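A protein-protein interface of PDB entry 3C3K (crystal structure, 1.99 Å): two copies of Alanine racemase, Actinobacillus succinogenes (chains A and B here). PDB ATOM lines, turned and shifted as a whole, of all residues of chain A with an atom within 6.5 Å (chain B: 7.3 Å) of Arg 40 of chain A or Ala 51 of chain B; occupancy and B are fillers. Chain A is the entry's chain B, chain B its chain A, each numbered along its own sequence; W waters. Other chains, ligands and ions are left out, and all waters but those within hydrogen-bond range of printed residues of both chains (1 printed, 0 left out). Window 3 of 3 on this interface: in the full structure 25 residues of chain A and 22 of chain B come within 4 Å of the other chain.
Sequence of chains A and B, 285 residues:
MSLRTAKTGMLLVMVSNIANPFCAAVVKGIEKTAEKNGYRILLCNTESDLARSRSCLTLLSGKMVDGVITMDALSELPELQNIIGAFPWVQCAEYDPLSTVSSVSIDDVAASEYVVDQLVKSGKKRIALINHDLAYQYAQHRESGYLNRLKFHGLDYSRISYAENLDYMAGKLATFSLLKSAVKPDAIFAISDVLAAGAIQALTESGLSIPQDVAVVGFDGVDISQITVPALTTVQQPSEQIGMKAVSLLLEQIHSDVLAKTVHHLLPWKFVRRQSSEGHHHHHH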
ATOM      1  N   THR A   8     -15.753 -32.767 -16.775  1.00  0.00           N
ATOM      2  CA  THR A   8     -14.735 -31.801 -17.207  1.00  0.00           C
ATOM      3  C   THR A   8     -13.816 -32.458 -18.235  1.00  0.00           C
ATOM      4  O   THR A   8     -13.245 -33.538 -17.997  1.00  0.00           O
ATOM      5  CB  THR A   8     -13.916 -31.212 -15.996  1.00  0.00           C
ATOM      6  OG1 THR A   8     -12.511 -31.190 -16.303  1.00  0.00           O
ATOM      7  CG2 THR A   8     -14.139 -32.020 -14.717  1.00  0.00           C
ATOM      8  N   GLY A   9     -13.699 -31.831 -19.397  1.00  0.00           N
ATOM      9  CA  GLY A   9     -12.834 -32.376 -20.432  1.00  0.00           C
ATOM     10  C   GLY A   9     -11.408 -31.901 -20.299  1.00  0.00           C
ATOM     11  O   GLY A   9     -11.091 -31.151 -19.409  1.00  0.00           O
ATOM     12  N   MET A  10     -10.557 -32.339 -21.220  1.00  0.00           N
ATOM     13  CA  MET A  10      -9.234 -31.775 -21.351  1.00  0.00           C
ATOM     14  C   MET A  10      -8.992 -31.441 -22.826  1.00  0.00           C
ATOM     15  O   MET A  10      -9.503 -32.108 -23.769  1.00  0.00           O
ATOM     16  CB  MET A  10      -8.120 -32.725 -20.818  1.00  0.00           C
ATOM     17  CG  MET A  10      -8.074 -32.896 -19.257  1.00  0.00           C
ATOM     18  SD  MET A  10      -6.623 -33.775 -18.552  1.00  0.00           S
ATOM     19  CE  MET A  10      -6.992 -35.457 -18.953  1.00  0.00           C
ATOM     20  N   LEU A  11      -8.182 -30.409 -23.009  1.00  0.00           N
ATOM     21  CA  LEU A  11      -7.641 -30.048 -24.312  1.00  0.00           C
ATOM     22  C   LEU A  11      -6.116 -30.224 -24.320  1.00  0.00           C
ATOM     23  O   LEU A  11      -5.452 -29.958 -23.293  1.00  0.00           O
ATOM     24  CB  LEU A  11      -7.998 -28.612 -24.597  1.00  0.00           C
ATOM     25  CG  LEU A  11      -9.433 -28.154 -24.322  1.00  0.00           C
ATOM     26  CD1 LEU A  11      -9.490 -26.698 -24.621  1.00  0.00           C
ATOM     27  CD2 LEU A  11     -10.415 -28.949 -25.237  1.00  0.00           C
ATOM     28  N   LEU A  12      -5.596 -30.709 -25.433  1.00  0.00           N
ATOM     29  CA  LEU A  12      -4.157 -30.813 -25.687  1.00  0.00           C
ATOM     30  C   LEU A  12      -3.584 -29.536 -26.336  1.00  0.00           C
ATOM     31  O   LEU A  12      -4.034 -29.109 -27.421  1.00  0.00           O
ATOM     32  CB  LEU A  12      -3.853 -32.039 -26.581  1.00  0.00           C
ATOM     33  CG  LEU A  12      -2.400 -32.249 -27.046  1.00  0.00           C
ATOM     34  CD1 LEU A  12      -1.439 -32.459 -25.845  1.00  0.00           C
ATOM     35  CD2 LEU A  12      -2.321 -33.436 -27.906  1.00  0.00           C
ATOM     36  N   ALA A  34     -10.347 -21.801 -21.630  1.00  0.00           N
ATOM     37  CA  ALA A  34     -10.706 -23.218 -21.471  1.00  0.00           C
ATOM     38  C   ALA A  34     -11.366 -23.456 -20.120  1.00  0.00           C
ATOM     39  O   ALA A  34     -12.400 -24.117 -20.071  1.00  0.00           O
ATOM     40  CB  ALA A  34      -9.472 -24.152 -21.698  1.00  0.00           C
ATOM     41  N   GLU A  35     -10.857 -22.850 -19.031  1.00  0.00           N
ATOM     42  CA  GLU A  35     -11.319 -23.230 -17.717  1.00  0.00           C
ATOM     43  C   GLU A  35     -12.668 -22.581 -17.354  1.00  0.00           C
ATOM     44  O   GLU A  35     -13.296 -23.004 -16.380  1.00  0.00           O
ATOM     45  CB  GLU A  35     -10.278 -22.932 -16.642  1.00  0.00           C
ATOM     46  CG  GLU A  35      -8.945 -23.633 -16.907  1.00  0.00           C
ATOM     47  CD  GLU A  35      -8.003 -23.726 -15.697  1.00  0.00           C
ATOM     48  OE1 GLU A  35      -7.736 -22.701 -15.055  1.00  0.00           O
ATOM     49  OE2 GLU A  35      -7.472 -24.819 -15.434  1.00  0.00           O
ATOM     50  N   GLY A  38     -15.255 -25.409 -18.896  1.00  0.00           N
ATOM     51  CA  GLY A  38     -15.311 -26.773 -18.392  1.00  0.00           C
ATOM     52  C   GLY A  38     -14.154 -27.617 -18.900  1.00  0.00           C
ATOM     53  O   GLY A  38     -14.237 -28.858 -18.982  1.00  0.00           O
ATOM     54  N   TYR A  39     -13.061 -26.976 -19.246  1.00  0.00           N
ATOM     55  CA  TYR A  39     -11.893 -27.745 -19.694  1.00  0.00           C
ATOM     56  C   TYR A  39     -10.691 -27.415 -18.871  1.00  0.00           C
ATOM     57  O   TYR A  39     -10.544 -26.282 -18.455  1.00  0.00           O
ATOM     58  CB  TYR A  39     -11.605 -27.437 -21.158  1.00  0.00           C
ATOM     59  CG  TYR A  39     -12.611 -28.056 -22.081  1.00  0.00           C
ATOM     60  CD1 TYR A  39     -12.441 -29.363 -22.553  1.00  0.00           C
ATOM     61  CD2 TYR A  39     -13.707 -27.339 -22.528  1.00  0.00           C
ATOM     62  CE1 TYR A  39     -13.371 -29.960 -23.369  1.00  0.00           C
ATOM     63  CE2 TYR A  39     -14.653 -27.940 -23.353  1.00  0.00           C
ATOM     64  CZ  TYR A  39     -14.443 -29.247 -23.784  1.00  0.00           C
ATOM     65  OH  TYR A  39     -15.340 -29.852 -24.621  1.00  0.00           O
ATOM     66  N   ARG A  40      -9.840 -28.419 -18.660  1.00  0.00           N
ATOM     67  CA  ARG A  40      -8.471 -28.235 -18.215  1.00  0.00           C
ATOM     68  C   ARG A  40      -7.487 -28.593 -19.348  1.00  0.00           C
ATOM     69  O   ARG A  40      -7.866 -29.171 -20.373  1.00  0.00           O
ATOM     70  CB  ARG A  40      -8.178 -29.132 -16.989  1.00  0.00           C
ATOM     71  CG  ARG A  40      -9.229 -29.066 -15.895  1.00  0.00           C
ATOM     72  CD  ARG A  40      -9.141 -27.707 -15.246  1.00  0.00           C
ATOM     73  NE  ARG A  40     -10.049 -27.579 -14.123  1.00  0.00           N
ATOM     74  CZ  ARG A  40     -10.037 -26.588 -13.242  1.00  0.00           C
ATOM     75  NH1 ARG A  40      -9.190 -25.565 -13.353  1.00  0.00           N
ATOM     76  NH2 ARG A  40     -10.943 -26.593 -12.286  1.00  0.00           N
ATOM     77  N   ILE A  41      -6.224 -28.263 -19.150  1.00  0.00           N
ATOM     78  CA  ILE A  41      -5.289 -28.198 -20.253  1.00  0.00           C
ATOM     79  C   ILE A  41      -4.139 -29.176 -20.048  1.00  0.00           C
ATOM     80  O   ILE A  41      -3.537 -29.208 -18.984  1.00  0.00           O
ATOM     81  CB  ILE A  41      -4.741 -26.729 -20.339  1.00  0.00           C
ATOM     82  CG1 ILE A  41      -5.883 -25.714 -20.663  1.00  0.00           C
ATOM     83  CG2 ILE A  41      -3.621 -26.603 -21.311  1.00  0.00           C
ATOM     84  CD1 ILE A  41      -6.536 -25.976 -22.004  1.00  0.00           C
ATOM     85  N   LEU A  42      -3.827 -29.984 -21.057  1.00  0.00           N
ATOM     86  CA  LEU A  42      -2.598 -30.768 -20.994  1.00  0.00           C
ATOM     87  C   LEU A  42      -1.636 -30.200 -22.017  1.00  0.00           C
ATOM     88  O   LEU A  42      -2.055 -29.870 -23.162  1.00  0.00           O
ATOM     89  CB  LEU A  42      -2.851 -32.220 -21.288  1.00  0.00           C
ATOM     90  CG  LEU A  42      -3.403 -33.165 -20.237  1.00  0.00           C
ATOM     91  CD1 LEU A  42      -3.598 -34.499 -20.932  1.00  0.00           C
ATOM     92  CD2 LEU A  42      -2.492 -33.287 -19.023  1.00  0.00           C
ATOM     93  N   CYS B  44       1.425 -30.815 -17.075  1.00  0.00           N
ATOM     94  CA  CYS B  44       0.270 -30.071 -16.621  1.00  0.00           C
ATOM     95  C   CYS B  44       0.771 -28.791 -15.870  1.00  0.00           C
ATOM     96  O   CYS B  44       1.477 -28.903 -14.898  1.00  0.00           O
ATOM     97  CB  CYS B  44      -0.619 -30.954 -15.717  1.00  0.00           C
ATOM     98  SG  CYS B  44      -2.208 -30.046 -15.341  1.00  0.00           S
ATOM     99  N   THR B  46      -0.021 -26.905 -13.260  1.00  0.00           N
ATOM    100  CA  THR B  46      -1.057 -27.025 -12.215  1.00  0.00           C
ATOM    101  C   THR B  46      -1.214 -25.774 -11.402  1.00  0.00           C
ATOM    102  O   THR B  46      -2.279 -25.504 -10.830  1.00  0.00           O
ATOM    103  CB  THR B  46      -0.735 -28.159 -11.244  1.00  0.00           C
ATOM    104  OG1 THR B  46       0.495 -27.844 -10.579  1.00  0.00           O
ATOM    105  CG2 THR B  46      -0.603 -29.437 -12.001  1.00  0.00           C
ATOM    106  N   SER B  48      -0.070 -25.707  -8.576  1.00  0.00           N
ATOM    107  CA  SER B  48      -0.469 -26.284  -7.289  1.00  0.00           C
ATOM    108  C   SER B  48      -1.941 -26.102  -6.966  1.00  0.00           C
ATOM    109  O   SER B  48      -2.307 -25.897  -5.812  1.00  0.00           O
ATOM    110  CB  SER B  48       0.397 -25.781  -6.133  1.00  0.00           C
ATOM    111  OG  SER B  48       1.764 -25.881  -6.488  1.00  0.00           O
ATOM    112  N   ASP B  49      -2.773 -26.253  -7.999  1.00  0.00           N
ATOM    113  CA  ASP B  49      -4.202 -26.163  -7.887  1.00  0.00           C
ATOM    114  C   ASP B  49      -4.755 -27.572  -8.094  1.00  0.00           C
ATOM    115  O   ASP B  49      -4.828 -28.062  -9.205  1.00  0.00           O
ATOM    116  CB  ASP B  49      -4.743 -25.234  -8.959  1.00  0.00           C
ATOM    117  CG  ASP B  49      -6.257 -25.234  -9.025  1.00  0.00           C
ATOM    118  OD1 ASP B  49      -6.895 -25.970  -8.266  1.00  0.00           O
ATOM    119  OD2 ASP B  49      -6.810 -24.476  -9.844  1.00  0.00           O
ATOM    120  N   LEU B  50      -5.176 -28.172  -6.994  1.00  0.00           N
ATOM    121  CA  LEU B  50      -5.584 -29.569  -6.909  1.00  0.00           C
ATOM    122  C   LEU B  50      -6.735 -29.805  -7.882  1.00  0.00           C
ATOM    123  O   LEU B  50      -6.862 -30.905  -8.348  1.00  0.00           O
ATOM    124  CB  LEU B  50      -6.020 -29.882  -5.464  1.00  0.00           C
ATOM    125  CG  LEU B  50      -6.473 -31.300  -5.108  1.00  0.00           C
ATOM    126  CD1 LEU B  50      -5.394 -32.294  -5.412  1.00  0.00           C
ATOM    127  CD2 LEU B  50      -6.900 -31.363  -3.612  1.00  0.00           C
ATOM    128  N   ALA B  51      -7.552 -28.780  -8.206  1.00  0.00           N
ATOM    129  CA  ALA B  51      -8.544 -28.952  -9.283  1.00  0.00           C
ATOM    130  C   ALA B  51      -7.919 -29.366 -10.638  1.00  0.00           C
ATOM    131  O   ALA B  51      -8.462 -30.230 -11.304  1.00  0.00           O
ATOM    132  CB  ALA B  51      -9.374 -27.750  -9.463  1.00  0.00           C
ATOM    133  N   ARG B  52      -6.809 -28.746 -11.043  1.00  0.00           N
ATOM    134  CA  ARG B  52      -6.073 -29.181 -12.239  1.00  0.00           C
ATOM    135  C   ARG B  52      -5.360 -30.488 -12.010  1.00  0.00           C
ATOM    136  O   ARG B  52      -5.315 -31.357 -12.874  1.00  0.00           O
ATOM    137  CB  ARG B  52      -5.058 -28.133 -12.657  1.00  0.00           C
ATOM    138  CG  ARG B  52      -5.661 -26.766 -12.934  1.00  0.00           C
ATOM    139  CD  ARG B  52      -4.515 -25.743 -13.230  1.00  0.00           C
ATOM    140  NE  ARG B  52      -5.066 -24.522 -13.796  1.00  0.00           N
ATOM    141  CZ  ARG B  52      -4.383 -23.418 -14.053  1.00  0.00           C
ATOM    142  NH1 ARG B  52      -3.071 -23.352 -13.838  1.00  0.00           N
ATOM    143  NH2 ARG B  52      -5.024 -22.383 -14.585  1.00  0.00           N
ATOM    144  N   SER B  53      -4.773 -30.656 -10.861  1.00  0.00           N
ATOM    145  CA  SER B  53      -4.140 -31.952 -10.586  1.00  0.00           C
ATOM    146  C   SER B  53      -5.092 -33.120 -10.693  1.00  0.00           C
ATOM    147  O   SER B  53      -4.709 -34.139 -11.263  1.00  0.00           O
ATOM    148  CB  SER B  53      -3.462 -31.997  -9.220  1.00  0.00           C
ATOM    149  OG  SER B  53      -2.514 -30.974  -9.140  1.00  0.00           O
ATOM    150  N   ARG B  54      -6.315 -32.990 -10.159  1.00  0.00           N
ATOM    151  CA  ARG B  54      -7.245 -34.131 -10.149  1.00  0.00           C
ATOM    152  C   ARG B  54      -7.607 -34.527 -11.579  1.00  0.00           C
ATOM    153  O   ARG B  54      -7.824 -35.711 -11.910  1.00  0.00           O
ATOM    154  CB  ARG B  54      -8.547 -33.786  -9.397  1.00  0.00           C
ATOM    155  CG  ARG B  54      -8.443 -33.819  -7.923  1.00  0.00           C
ATOM    156  CD  ARG B  54      -9.852 -33.890  -7.299  1.00  0.00           C
ATOM    157  NE  ARG B  54      -9.792 -33.714  -5.850  1.00  0.00           N
ATOM    158  CZ  ARG B  54      -9.561 -34.703  -4.972  1.00  0.00           C
ATOM    159  NH1 ARG B  54      -9.340 -35.946  -5.398  1.00  0.00           N
ATOM    160  NH2 ARG B  54      -9.549 -34.455  -3.659  1.00  0.00           N
ATOM    161  N   SER B  55      -7.642 -33.514 -12.436  1.00  0.00           N
ATOM    162  CA  SER B  55      -7.980 -33.686 -13.804  1.00  0.00           C
ATOM    163  C   SER B  55      -6.842 -34.418 -14.511  1.00  0.00           C
ATOM    164  O   SER B  55      -7.043 -35.471 -15.121  1.00  0.00           O
ATOM    165  CB  SER B  55      -8.235 -32.298 -14.391  1.00  0.00           C
ATOM    166  OG  SER B  55      -8.792 -32.367 -15.689  1.00  0.00           O
ATOM    167  N   CYS B  56      -5.624 -33.896 -14.432  1.00  0.00           N
ATOM    168  CA  CYS B  56      -4.523 -34.547 -15.158  1.00  0.00           C
ATOM    169  C   CYS B  56      -4.165 -35.891 -14.580  1.00  0.00           C
ATOM    170  O   CYS B  56      -3.654 -36.773 -15.302  1.00  0.00           O
ATOM    171  CB  CYS B  56      -3.288 -33.635 -15.290  1.00  0.00           C
ATOM    172  SG  CYS B  56      -2.493 -33.233 -13.739  1.00  0.00           S
ATOM    173  N   GLU B  76      -0.152 -29.161  -1.034  1.00  0.00           N
ATOM    174  CA  GLU B  76      -1.056 -29.979  -1.877  1.00  0.00           C
ATOM    175  C   GLU B  76      -0.656 -31.436  -1.764  1.00  0.00           C
ATOM    176  O   GLU B  76      -1.429 -32.308  -2.128  1.00  0.00           O
ATOM    177  CB  GLU B  76      -0.965 -29.538  -3.372  1.00  0.00           C
ATOM    178  CG  GLU B  76      -2.070 -30.062  -4.299  1.00  0.00           C
ATOM    179  CD  GLU B  76      -1.713 -29.921  -5.791  1.00  0.00           C
ATOM    180  OE1 GLU B  76      -0.598 -29.472  -6.063  1.00  0.00           O
ATOM    181  OE2 GLU B  76      -2.519 -30.266  -6.695  1.00  0.00           O
HETATM  182  O   HOH W   1      -8.983 -24.054 -10.805  1.00  0.00           O
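The guanidinium group (NH2) of Arg 52 of chain B lies within salt-bridge range of the side-chain carboxylate (OE1) of Glu 35 of chain A.
OE2 of Glu 35 of chain A lies within salt-bridge range of NH1 of Arg 40 of chain A (2.8 Å).
O of Leu 11 of chain A sits at hydrogen-bond distance from N of Leu 42 of chain A, at 2.8 Å.
OD1 of Asp 49 of chain B lies within hydrogen-bond range of N of Ala 51 of chain B (2.9 Å).
The side-chain sulfur (SG) of Cys 56 of chain B lies close to the side-chain sulfur (SG) of Cys 44 of chain B (3.6 Å).
O of Arg 52 of chain B lies within hydrogen-bond range of SG of Cys 56 of chain B, 3.5 Å away.
O of Gly 9 of chain A lies within hydrogen-bond range of N of Arg 40 of chain A, 3.1 Å away.
Ser 55 of chain B touches Thr 8 of chain A (OG to OG1, 3.9 Å).
Met 10 of chain A touches Ser 55 of chain B.
CB of Ala 51 of chain B touches NH2 of Arg 40 of chain A, at 3.4 Å.
Arg 40 of chain A touches Arg 52 of chain B.
Ser 55 of chain B touches Arg 40 of chain A (OG to CG, 3.3 Å).
O of Ile 41 of chain A touches SG of Cys 44 of chain B (3.97 Å).
CB of Cys 56 of chain B touches CD2 of Leu 42 of chain A, at 3.8 Å.
Of the printed residues of chain B, Thr 8 of chain A touches Ser 55 (3.9 Å).
Printed residues of chain B within 4 Å of Arg 40 of chain A: Ala 51, Arg 52 and Ser 55.
Of the printed residues of chain B, Leu 42 of chain A touches Cys 56 (3.8 Å).
Ala 51 of chain B touches just one residue of chain A: Arg 40 (3.4 Å).
Printed residues of chain A within 4 Å of Cys 56 of chain B: Leu 42 (3.8 Å).
The nearest residue of chain B that does not touch Arg 40 of chain A is Asp 49 of chain B (4.4 Å).
The nearest printed residue of chain A that does not touch Ala 51 of chain B is Thr 8 of chain A (6.5 Å).
Hydrophobic or aromatic side chains of chain A that line the printed part of chain B: Met 10 and Leu 42.
Along chain A the printed residues that touch a printed residue of chain B span positions 8 to 42.
Of the 12 printed residues of chain B, 5 touch a printed residue of chain A.
Among the printed residues, 8 pairs touch across the chains.
Among the printed residues, Asp or Glu carboxylates within 4 Å of a Lys or Arg side-chain nitrogen of the other chain: Glu 35 of chain A with Arg 52 of chain B (2.8 Å).
No position is printed for both chains.
Water W1 bridges the side-chain carboxylate (OD2) of Asp 49 of chain B (2.4 Å) and the guanidinium group (NH1) of Arg 40 of chain A (3.0 Å).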
